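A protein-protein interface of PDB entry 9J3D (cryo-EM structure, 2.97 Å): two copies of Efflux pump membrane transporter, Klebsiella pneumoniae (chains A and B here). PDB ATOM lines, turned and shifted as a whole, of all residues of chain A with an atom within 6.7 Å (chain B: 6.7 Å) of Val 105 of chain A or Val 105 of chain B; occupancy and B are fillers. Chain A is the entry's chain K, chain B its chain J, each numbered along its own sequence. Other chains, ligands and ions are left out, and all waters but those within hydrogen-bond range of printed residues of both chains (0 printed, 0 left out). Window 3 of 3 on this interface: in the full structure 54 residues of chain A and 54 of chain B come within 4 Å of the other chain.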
ATOM      1  N   PRO A 100     -18.602 -11.734 -10.593  1.00  0.00           N
ATOM      2  CA  PRO A 100     -17.525 -11.199  -9.750  1.00  0.00           C
ATOM      3  C   PRO A 100     -16.265 -12.047  -9.752  1.00  0.00           C
ATOM      4  O   PRO A 100     -15.179 -11.527  -9.458  1.00  0.00           O
ATOM      5  CB  PRO A 100     -18.172 -11.148  -8.359  1.00  0.00           C
ATOM      6  CG  PRO A 100     -19.652 -11.346  -8.592  1.00  0.00           C
ATOM      7  CD  PRO A 100     -19.731 -12.221  -9.791  1.00  0.00           C
ATOM      8  N   GLU A 101     -16.371 -13.337 -10.075  1.00  0.00           N
ATOM      9  CA  GLU A 101     -15.225 -14.227  -9.927  1.00  0.00           C
ATOM     10  C   GLU A 101     -14.115 -13.889 -10.916  1.00  0.00           C
ATOM     11  O   GLU A 101     -12.932 -13.896 -10.548  1.00  0.00           O
ATOM     12  CB  GLU A 101     -15.665 -15.682 -10.080  1.00  0.00           C
ATOM     13  CG  GLU A 101     -14.531 -16.685  -9.943  1.00  0.00           C
ATOM     14  CD  GLU A 101     -14.416 -17.250  -8.539  1.00  0.00           C
ATOM     15  OE1 GLU A 101     -13.866 -18.362  -8.385  1.00  0.00           O
ATOM     16  OE2 GLU A 101     -14.872 -16.582  -7.589  1.00  0.00           O
ATOM     17  N   LEU A 102     -14.490 -13.591 -12.167  1.00  0.00           N
ATOM     18  CA  LEU A 102     -13.489 -13.229 -13.213  1.00  0.00           C
ATOM     19  C   LEU A 102     -12.813 -11.912 -12.817  1.00  0.00           C
ATOM     20  O   LEU A 102     -11.610 -11.761 -13.097  1.00  0.00           O
ATOM     21  CB  LEU A 102     -14.184 -13.162 -14.577  1.00  0.00           C
ATOM     22  CG  LEU A 102     -14.124 -11.826 -15.316  1.00  0.00           C
ATOM     23  CD1 LEU A 102     -13.680 -12.022 -16.756  1.00  0.00           C
ATOM     24  CD2 LEU A 102     -15.476 -11.136 -15.280  1.00  0.00           C
ATOM     25  N   ALA A 103     -13.551 -10.998 -12.187  1.00  0.00           N
ATOM     26  CA  ALA A 103     -12.982  -9.752 -11.690  1.00  0.00           C
ATOM     27  C   ALA A 103     -11.976 -10.024 -10.584  1.00  0.00           C
ATOM     28  O   ALA A 103     -10.881  -9.452 -10.571  1.00  0.00           O
ATOM     29  CB  ALA A 103     -14.097  -8.831 -11.193  1.00  0.00           C
ATOM     30  N   GLN A 104     -12.325 -10.913  -9.654  1.00  0.00           N
ATOM     31  CA  GLN A 104     -11.423 -11.207  -8.546  1.00  0.00           C
ATOM     32  C   GLN A 104     -10.131 -11.852  -9.039  1.00  0.00           C
ATOM     33  O   GLN A 104      -9.033 -11.480  -8.599  1.00  0.00           O
ATOM     34  CB  GLN A 104     -12.130 -12.101  -7.531  1.00  0.00           C
ATOM     35  CG  GLN A 104     -11.240 -13.114  -6.882  1.00  0.00           C
ATOM     36  CD  GLN A 104     -11.966 -13.990  -5.872  1.00  0.00           C
ATOM     37  OE1 GLN A 104     -12.208 -15.174  -6.119  1.00  0.00           O
ATOM     38  NE2 GLN A 104     -12.288 -13.421  -4.719  1.00  0.00           N
ATOM     39  N   VAL A 105     -10.235 -12.815  -9.960  1.00  0.00           N
ATOM     40  CA  VAL A 105      -9.020 -13.486 -10.414  1.00  0.00           C
ATOM     41  C   VAL A 105      -8.158 -12.526 -11.222  1.00  0.00           C
ATOM     42  O   VAL A 105      -6.930 -12.559 -11.130  1.00  0.00           O
ATOM     43  CB  VAL A 105      -9.333 -14.774 -11.204  1.00  0.00           C
ATOM     44  CG1 VAL A 105      -9.629 -15.927 -10.252  1.00  0.00           C
ATOM     45  CG2 VAL A 105     -10.436 -14.572 -12.198  1.00  0.00           C
ATOM     46  N   ASP A 106      -8.782 -11.644 -12.011  1.00  0.00           N
ATOM     47  CA  ASP A 106      -8.011 -10.635 -12.736  1.00  0.00           C
ATOM     48  C   ASP A 106      -7.295  -9.683 -11.781  1.00  0.00           C
ATOM     49  O   ASP A 106      -6.122  -9.337 -11.991  1.00  0.00           O
ATOM     50  CB  ASP A 106      -8.935  -9.855 -13.672  1.00  0.00           C
ATOM     51  CG  ASP A 106      -8.179  -9.119 -14.757  1.00  0.00           C
ATOM     52  OD1 ASP A 106      -7.407  -9.768 -15.492  1.00  0.00           O
ATOM     53  OD2 ASP A 106      -8.353  -7.887 -14.871  1.00  0.00           O
ATOM     54  N   VAL A 107      -7.989  -9.248 -10.727  1.00  0.00           N
ATOM     55  CA  VAL A 107      -7.390  -8.328  -9.765  1.00  0.00           C
ATOM     56  C   VAL A 107      -6.188  -8.977  -9.090  1.00  0.00           C
ATOM     57  O   VAL A 107      -5.124  -8.362  -8.956  1.00  0.00           O
ATOM     58  CB  VAL A 107      -8.440  -7.865  -8.740  1.00  0.00           C
ATOM     59  CG1 VAL A 107      -7.770  -7.190  -7.561  1.00  0.00           C
ATOM     60  CG2 VAL A 107      -9.434  -6.915  -9.392  1.00  0.00           C
ATOM     61  N   GLN A 108      -6.330 -10.237  -8.674  1.00  0.00           N
ATOM     62  CA  GLN A 108      -5.203 -10.913  -8.038  1.00  0.00           C
ATOM     63  C   GLN A 108      -4.100 -11.182  -9.058  1.00  0.00           C
ATOM     64  O   GLN A 108      -2.908 -11.135  -8.732  1.00  0.00           O
ATOM     65  CB  GLN A 108      -5.704 -12.186  -7.342  1.00  0.00           C
ATOM     66  CG  GLN A 108      -4.855 -12.747  -6.179  1.00  0.00           C
ATOM     67  CD  GLN A 108      -3.394 -13.033  -6.470  1.00  0.00           C
ATOM     68  OE1 GLN A 108      -3.006 -13.287  -7.603  1.00  0.00           O
ATOM     69  NE2 GLN A 108      -2.570 -12.965  -5.434  1.00  0.00           N
ATOM     70  N   ASN A 109      -4.479 -11.409 -10.313  1.00  0.00           N
ATOM     71  CA  ASN A 109      -3.502 -11.626 -11.367  1.00  0.00           C
ATOM     72  C   ASN A 109      -2.615 -10.405 -11.553  1.00  0.00           C
ATOM     73  O   ASN A 109      -1.413 -10.539 -11.813  1.00  0.00           O
ATOM     74  CB  ASN A 109      -4.252 -11.971 -12.650  1.00  0.00           C
ATOM     75  CG  ASN A 109      -4.190 -13.441 -12.973  1.00  0.00           C
ATOM     76  OD1 ASN A 109      -3.196 -14.098 -12.706  1.00  0.00           O
ATOM     77  ND2 ASN A 109      -5.308 -13.991 -13.422  1.00  0.00           N
ATOM     78  N   ARG A 110      -3.191  -9.211 -11.426  1.00  0.00           N
ATOM     79  CA  ARG A 110      -2.386  -7.991 -11.459  1.00  0.00           C
ATOM     80  C   ARG A 110      -1.635  -7.773 -10.145  1.00  0.00           C
ATOM     81  O   ARG A 110      -0.509  -7.252 -10.140  1.00  0.00           O
ATOM     82  CB  ARG A 110      -3.280  -6.795 -11.780  1.00  0.00           C
ATOM     83  CG  ARG A 110      -3.975  -6.935 -13.120  1.00  0.00           C
ATOM     84  CD  ARG A 110      -5.266  -6.147 -13.186  1.00  0.00           C
ATOM     85  NE  ARG A 110      -6.001  -6.458 -14.405  1.00  0.00           N
ATOM     86  CZ  ARG A 110      -5.713  -5.958 -15.599  1.00  0.00           C
ATOM     87  NH1 ARG A 110      -4.728  -5.093 -15.766  1.00  0.00           N
ATOM     88  NH2 ARG A 110      -6.435  -6.334 -16.649  1.00  0.00           N
ATOM     89  N   ILE B  43      -1.436 -16.993 -24.732  1.00  0.00           N
ATOM     90  CA  ILE B  43      -0.956 -16.415 -23.487  1.00  0.00           C
ATOM     91  C   ILE B  43       0.552 -16.272 -23.620  1.00  0.00           C
ATOM     92  O   ILE B  43       1.201 -17.088 -24.286  1.00  0.00           O
ATOM     93  CB  ILE B  43      -1.347 -17.264 -22.267  1.00  0.00           C
ATOM     94  CG1 ILE B  43      -1.636 -16.360 -21.072  1.00  0.00           C
ATOM     95  CG2 ILE B  43      -0.261 -18.260 -21.918  1.00  0.00           C
ATOM     96  CD1 ILE B  43      -2.717 -15.340 -21.331  1.00  0.00           C
ATOM     97  N   PRO B 100     -10.404 -16.857 -22.965  1.00  0.00           N
ATOM     98  CA  PRO B 100      -9.046 -16.428 -22.611  1.00  0.00           C
ATOM     99  C   PRO B 100      -8.825 -16.256 -21.121  1.00  0.00           C
ATOM    100  O   PRO B 100      -7.719 -16.532 -20.632  1.00  0.00           O
ATOM    101  CB  PRO B 100      -8.910 -15.099 -23.364  1.00  0.00           C
ATOM    102  CG  PRO B 100      -9.948 -15.139 -24.437  1.00  0.00           C
ATOM    103  CD  PRO B 100     -11.083 -15.903 -23.853  1.00  0.00           C
ATOM    104  N   GLU B 101      -9.841 -15.795 -20.386  1.00  0.00           N
ATOM    105  CA  GLU B 101      -9.668 -15.542 -18.963  1.00  0.00           C
ATOM    106  C   GLU B 101      -9.333 -16.827 -18.235  1.00  0.00           C
ATOM    107  O   GLU B 101      -8.429 -16.848 -17.384  1.00  0.00           O
ATOM    108  CB  GLU B 101     -10.929 -14.904 -18.382  1.00  0.00           C
ATOM    109  CG  GLU B 101     -10.826 -14.525 -16.912  1.00  0.00           C
ATOM    110  CD  GLU B 101     -10.250 -13.139 -16.698  1.00  0.00           C
ATOM    111  OE1 GLU B 101     -10.310 -12.638 -15.555  1.00  0.00           O
ATOM    112  OE2 GLU B 101      -9.735 -12.550 -17.672  1.00  0.00           O
ATOM    113  N   LEU B 102     -10.009 -17.933 -18.595  1.00  0.00           N
ATOM    114  CA  LEU B 102      -9.720 -19.152 -17.843  1.00  0.00           C
ATOM    115  C   LEU B 102      -8.338 -19.680 -18.190  1.00  0.00           C
ATOM    116  O   LEU B 102      -7.660 -20.246 -17.328  1.00  0.00           O
ATOM    117  CB  LEU B 102     -10.737 -20.291 -18.011  1.00  0.00           C
ATOM    118  CG  LEU B 102     -12.226 -20.074 -17.772  1.00  0.00           C
ATOM    119  CD1 LEU B 102     -12.929 -21.189 -18.409  1.00  0.00           C
ATOM    120  CD2 LEU B 102     -12.637 -19.907 -16.461  1.00  0.00           C
ATOM    121  N   ALA B 103      -7.898 -19.500 -19.437  1.00  0.00           N
ATOM    122  CA  ALA B 103      -6.568 -19.955 -19.823  1.00  0.00           C
ATOM    123  C   ALA B 103      -5.486 -19.185 -19.077  1.00  0.00           C
ATOM    124  O   ALA B 103      -4.544 -19.779 -18.537  1.00  0.00           O
ATOM    125  CB  ALA B 103      -6.401 -19.810 -21.332  1.00  0.00           C
ATOM    126  N   GLN B 104      -5.606 -17.855 -19.038  1.00  0.00           N
ATOM    127  CA  GLN B 104      -4.645 -17.052 -18.286  1.00  0.00           C
ATOM    128  C   GLN B 104      -4.671 -17.428 -16.813  1.00  0.00           C
ATOM    129  O   GLN B 104      -3.629 -17.459 -16.144  1.00  0.00           O
ATOM    130  CB  GLN B 104      -4.943 -15.565 -18.516  1.00  0.00           C
ATOM    131  CG  GLN B 104      -4.262 -14.538 -17.626  1.00  0.00           C
ATOM    132  CD  GLN B 104      -4.912 -14.302 -16.292  1.00  0.00           C
ATOM    133  OE1 GLN B 104      -5.588 -15.157 -15.716  1.00  0.00           O
ATOM    134  NE2 GLN B 104      -4.749 -13.081 -15.811  1.00  0.00           N
ATOM    135  N   VAL B 105      -5.864 -17.713 -16.299  1.00  0.00           N
ATOM    136  CA  VAL B 105      -6.028 -18.182 -14.933  1.00  0.00           C
ATOM    137  C   VAL B 105      -5.217 -19.446 -14.682  1.00  0.00           C
ATOM    138  O   VAL B 105      -4.469 -19.534 -13.700  1.00  0.00           O
ATOM    139  CB  VAL B 105      -7.526 -18.401 -14.670  1.00  0.00           C
ATOM    140  CG1 VAL B 105      -7.703 -19.456 -13.669  1.00  0.00           C
ATOM    141  CG2 VAL B 105      -8.171 -17.104 -14.187  1.00  0.00           C
ATOM    142  N   ASP B 106      -5.355 -20.443 -15.556  1.00  0.00           N
ATOM    143  CA  ASP B 106      -4.634 -21.698 -15.367  1.00  0.00           C
ATOM    144  C   ASP B 106      -3.128 -21.482 -15.463  1.00  0.00           C
ATOM    145  O   ASP B 106      -2.349 -22.071 -14.697  1.00  0.00           O
ATOM    146  CB  ASP B 106      -5.101 -22.724 -16.399  1.00  0.00           C
ATOM    147  CG  ASP B 106      -4.835 -24.151 -15.965  1.00  0.00           C
ATOM    148  OD1 ASP B 106      -5.300 -24.538 -14.873  1.00  0.00           O
ATOM    149  OD2 ASP B 106      -4.164 -24.887 -16.719  1.00  0.00           O
ATOM    150  N   VAL B 107      -2.706 -20.627 -16.397  1.00  0.00           N
ATOM    151  CA  VAL B 107      -1.283 -20.351 -16.570  1.00  0.00           C
ATOM    152  C   VAL B 107      -0.700 -19.744 -15.300  1.00  0.00           C
ATOM    153  O   VAL B 107       0.378 -20.138 -14.845  1.00  0.00           O
ATOM    154  CB  VAL B 107      -1.062 -19.439 -17.789  1.00  0.00           C
ATOM    155  CG1 VAL B 107       0.368 -18.936 -17.821  1.00  0.00           C
ATOM    156  CG2 VAL B 107      -1.393 -20.189 -19.065  1.00  0.00           C
ATOM    157  N   GLN B 108      -1.406 -18.783 -14.700  1.00  0.00           N
ATOM    158  CA  GLN B 108      -0.890 -18.176 -13.475  1.00  0.00           C
ATOM    159  C   GLN B 108      -0.960 -19.157 -12.308  1.00  0.00           C
ATOM    160  O   GLN B 108      -0.090 -19.154 -11.426  1.00  0.00           O
ATOM    161  CB  GLN B 108      -1.652 -16.888 -13.168  1.00  0.00           C
ATOM    162  CG  GLN B 108      -0.879 -15.875 -12.324  1.00  0.00           C
ATOM    163  CD  GLN B 108      -0.605 -16.321 -10.907  1.00  0.00           C
ATOM    164  OE1 GLN B 108      -1.397 -17.042 -10.300  1.00  0.00           O
ATOM    165  NE2 GLN B 108       0.526 -15.887 -10.366  1.00  0.00           N
ATOM    166  N   ASN B 109      -1.986 -20.010 -12.291  1.00  0.00           N
ATOM    167  CA  ASN B 109      -2.072 -21.040 -11.264  1.00  0.00           C
ATOM    168  C   ASN B 109      -0.849 -21.943 -11.288  1.00  0.00           C
ATOM    169  O   ASN B 109      -0.353 -22.347 -10.230  1.00  0.00           O
ATOM    170  CB  ASN B 109      -3.348 -21.861 -11.463  1.00  0.00           C
ATOM    171  CG  ASN B 109      -4.271 -21.803 -10.263  1.00  0.00           C
ATOM    172  OD1 ASN B 109      -3.822 -21.839  -9.120  1.00  0.00           O
ATOM    173  ND2 ASN B 109      -5.571 -21.706 -10.520  1.00  0.00           N
ATOM    174  N   ARG B 110      -0.354 -22.272 -12.480  1.00  0.00           N
ATOM    175  CA  ARG B 110       0.869 -23.067 -12.577  1.00  0.00           C
ATOM    176  C   ARG B 110       2.119 -22.232 -12.305  1.00  0.00           C
ATOM    177  O   ARG B 110       3.113 -22.741 -11.766  1.00  0.00           O
ATOM    178  CB  ARG B 110       0.946 -23.730 -13.949  1.00  0.00           C
ATOM    179  CG  ARG B 110      -0.201 -24.687 -14.197  1.00  0.00           C
ATOM    180  CD  ARG B 110      -0.524 -24.816 -15.668  1.00  0.00           C
ATOM    181  NE  ARG B 110      -1.791 -25.507 -15.858  1.00  0.00           N
ATOM    182  CZ  ARG B 110      -1.935 -26.824 -15.813  1.00  0.00           C
ATOM    183  NH1 ARG B 110      -0.902 -27.625 -15.614  1.00  0.00           N
ATOM    184  NH2 ARG B 110      -3.145 -27.349 -15.973  1.00  0.00           N
ATOM    185  N   GLN B 131      -2.371 -11.613 -21.850  1.00  0.00           N
ATOM    186  CA  GLN B 131      -3.129 -12.076 -23.003  1.00  0.00           C
ATOM    187  C   GLN B 131      -2.517 -11.498 -24.269  1.00  0.00           C
ATOM    188  O   GLN B 131      -2.437 -10.274 -24.418  1.00  0.00           O
ATOM    189  CB  GLN B 131      -4.583 -11.640 -22.875  1.00  0.00           C
ATOM    190  CG  GLN B 131      -5.267 -12.109 -21.615  1.00  0.00           C
ATOM    191  CD  GLN B 131      -6.222 -13.233 -21.900  1.00  0.00           C
ATOM    192  OE1 GLN B 131      -6.332 -13.677 -23.038  1.00  0.00           O
ATOM    193  NE2 GLN B 131      -6.921 -13.702 -20.873  1.00  0.00           N
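Glu 101 of chain B touches Val 105 of chain A (OE1 to CG2, 3.9 Å).
Val 105 of chain B touches Val 105 of chain A.
Asp 106 of chain A touches Glu 101 of chain B (CB to OE1, 3.6 Å).
Asn 109 of chain A touches Gln 108 of chain B (OD1 to CG, 2.9 Å).
Of the 11 printed residues of chain A, 4 touch a printed residue of chain B.
Printed residues of chain A that touch a printed residue of chain B: Leu 102, Val 105, Asp 106 and Asn 109.
Hydrophobic or aromatic side chains of chain A within 4 Å of the printed part of chain B: Leu 102 and Val 105.
Printed residues of chain B that touch a printed residue of chain A: Glu 101, Gln 104, Val 105 and Gln 108.
Among the printed residues, no Asp or Glu carboxylate lies within 4 Å of a Lys or Arg side-chain nitrogen of the other chain.
The side-chain amide oxygen of Gln 104 of chain B is in hydrogen-bond range of the side-chain amide nitrogen of Asn 109 of chain A (2.6 Å).
The backbone carbonyl oxygen (O) of Leu 102 of chain A lies close to the side-chain carboxylate (OE1) of Glu 101 of chain B (2.9 Å).
The side-chain carboxylate (OD2) of Asp 106 of chain A is in salt-bridge range of the guanidinium group (NE) of Arg 110 of chain A, 2.8 Å away.
The backbone carbonyl oxygen of Val 105 of chain A sits close to the side-chain amide nitrogen of Asn 109 of chain A (3.2 Å).
Val 105 of chain A touches Glu 101 of chain B, but with the chains exchanged Glu 101 of chain A does not touch Val 105 of chain B (6.8 Å).
Val 105 of chain A touches its own counterpart, Val 105 of chain B.
Asn 109 of chain A touches Gln 104 of chain B, but with the chains exchanged Gln 104 of chain A does not touch Asn 109 of chain B (10.3 Å).
Asn 109 of chain A touches Gln 108 of chain B, but with the chains exchanged Gln 108 of chain A does not touch Asn 109 of chain B (8.3 Å).
11 positions are printed for both chains.
Val 105 of chain A touches just these residues of chain B: Glu 101 (3.9 Å) and Val 105 (3.9 Å).
Of chain A, only Val 105 comes within 4 Å of Val 105 of chain B.
Printed residues of chain B within 4 Å of Leu 102 of chain A: Glu 101.
Of the printed residues of chain A, Glu 101 of chain B touches Leu 102, Val 105 and Asp 106.
Val 107 of chain B touches none of the printed residues of chain A.
The nearest residue of chain B that does not touch Val 105 of chain A is Gln 104 of chain B (5.2 Å).
The nearest residue of chain A that does not touch Val 105 of chain B is Asn 109 of chain A (4.3 Å).
The nearest printed residue of chain B that does not touch Leu 102 of chain A is Val 105 of chain B (6.4 Å).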
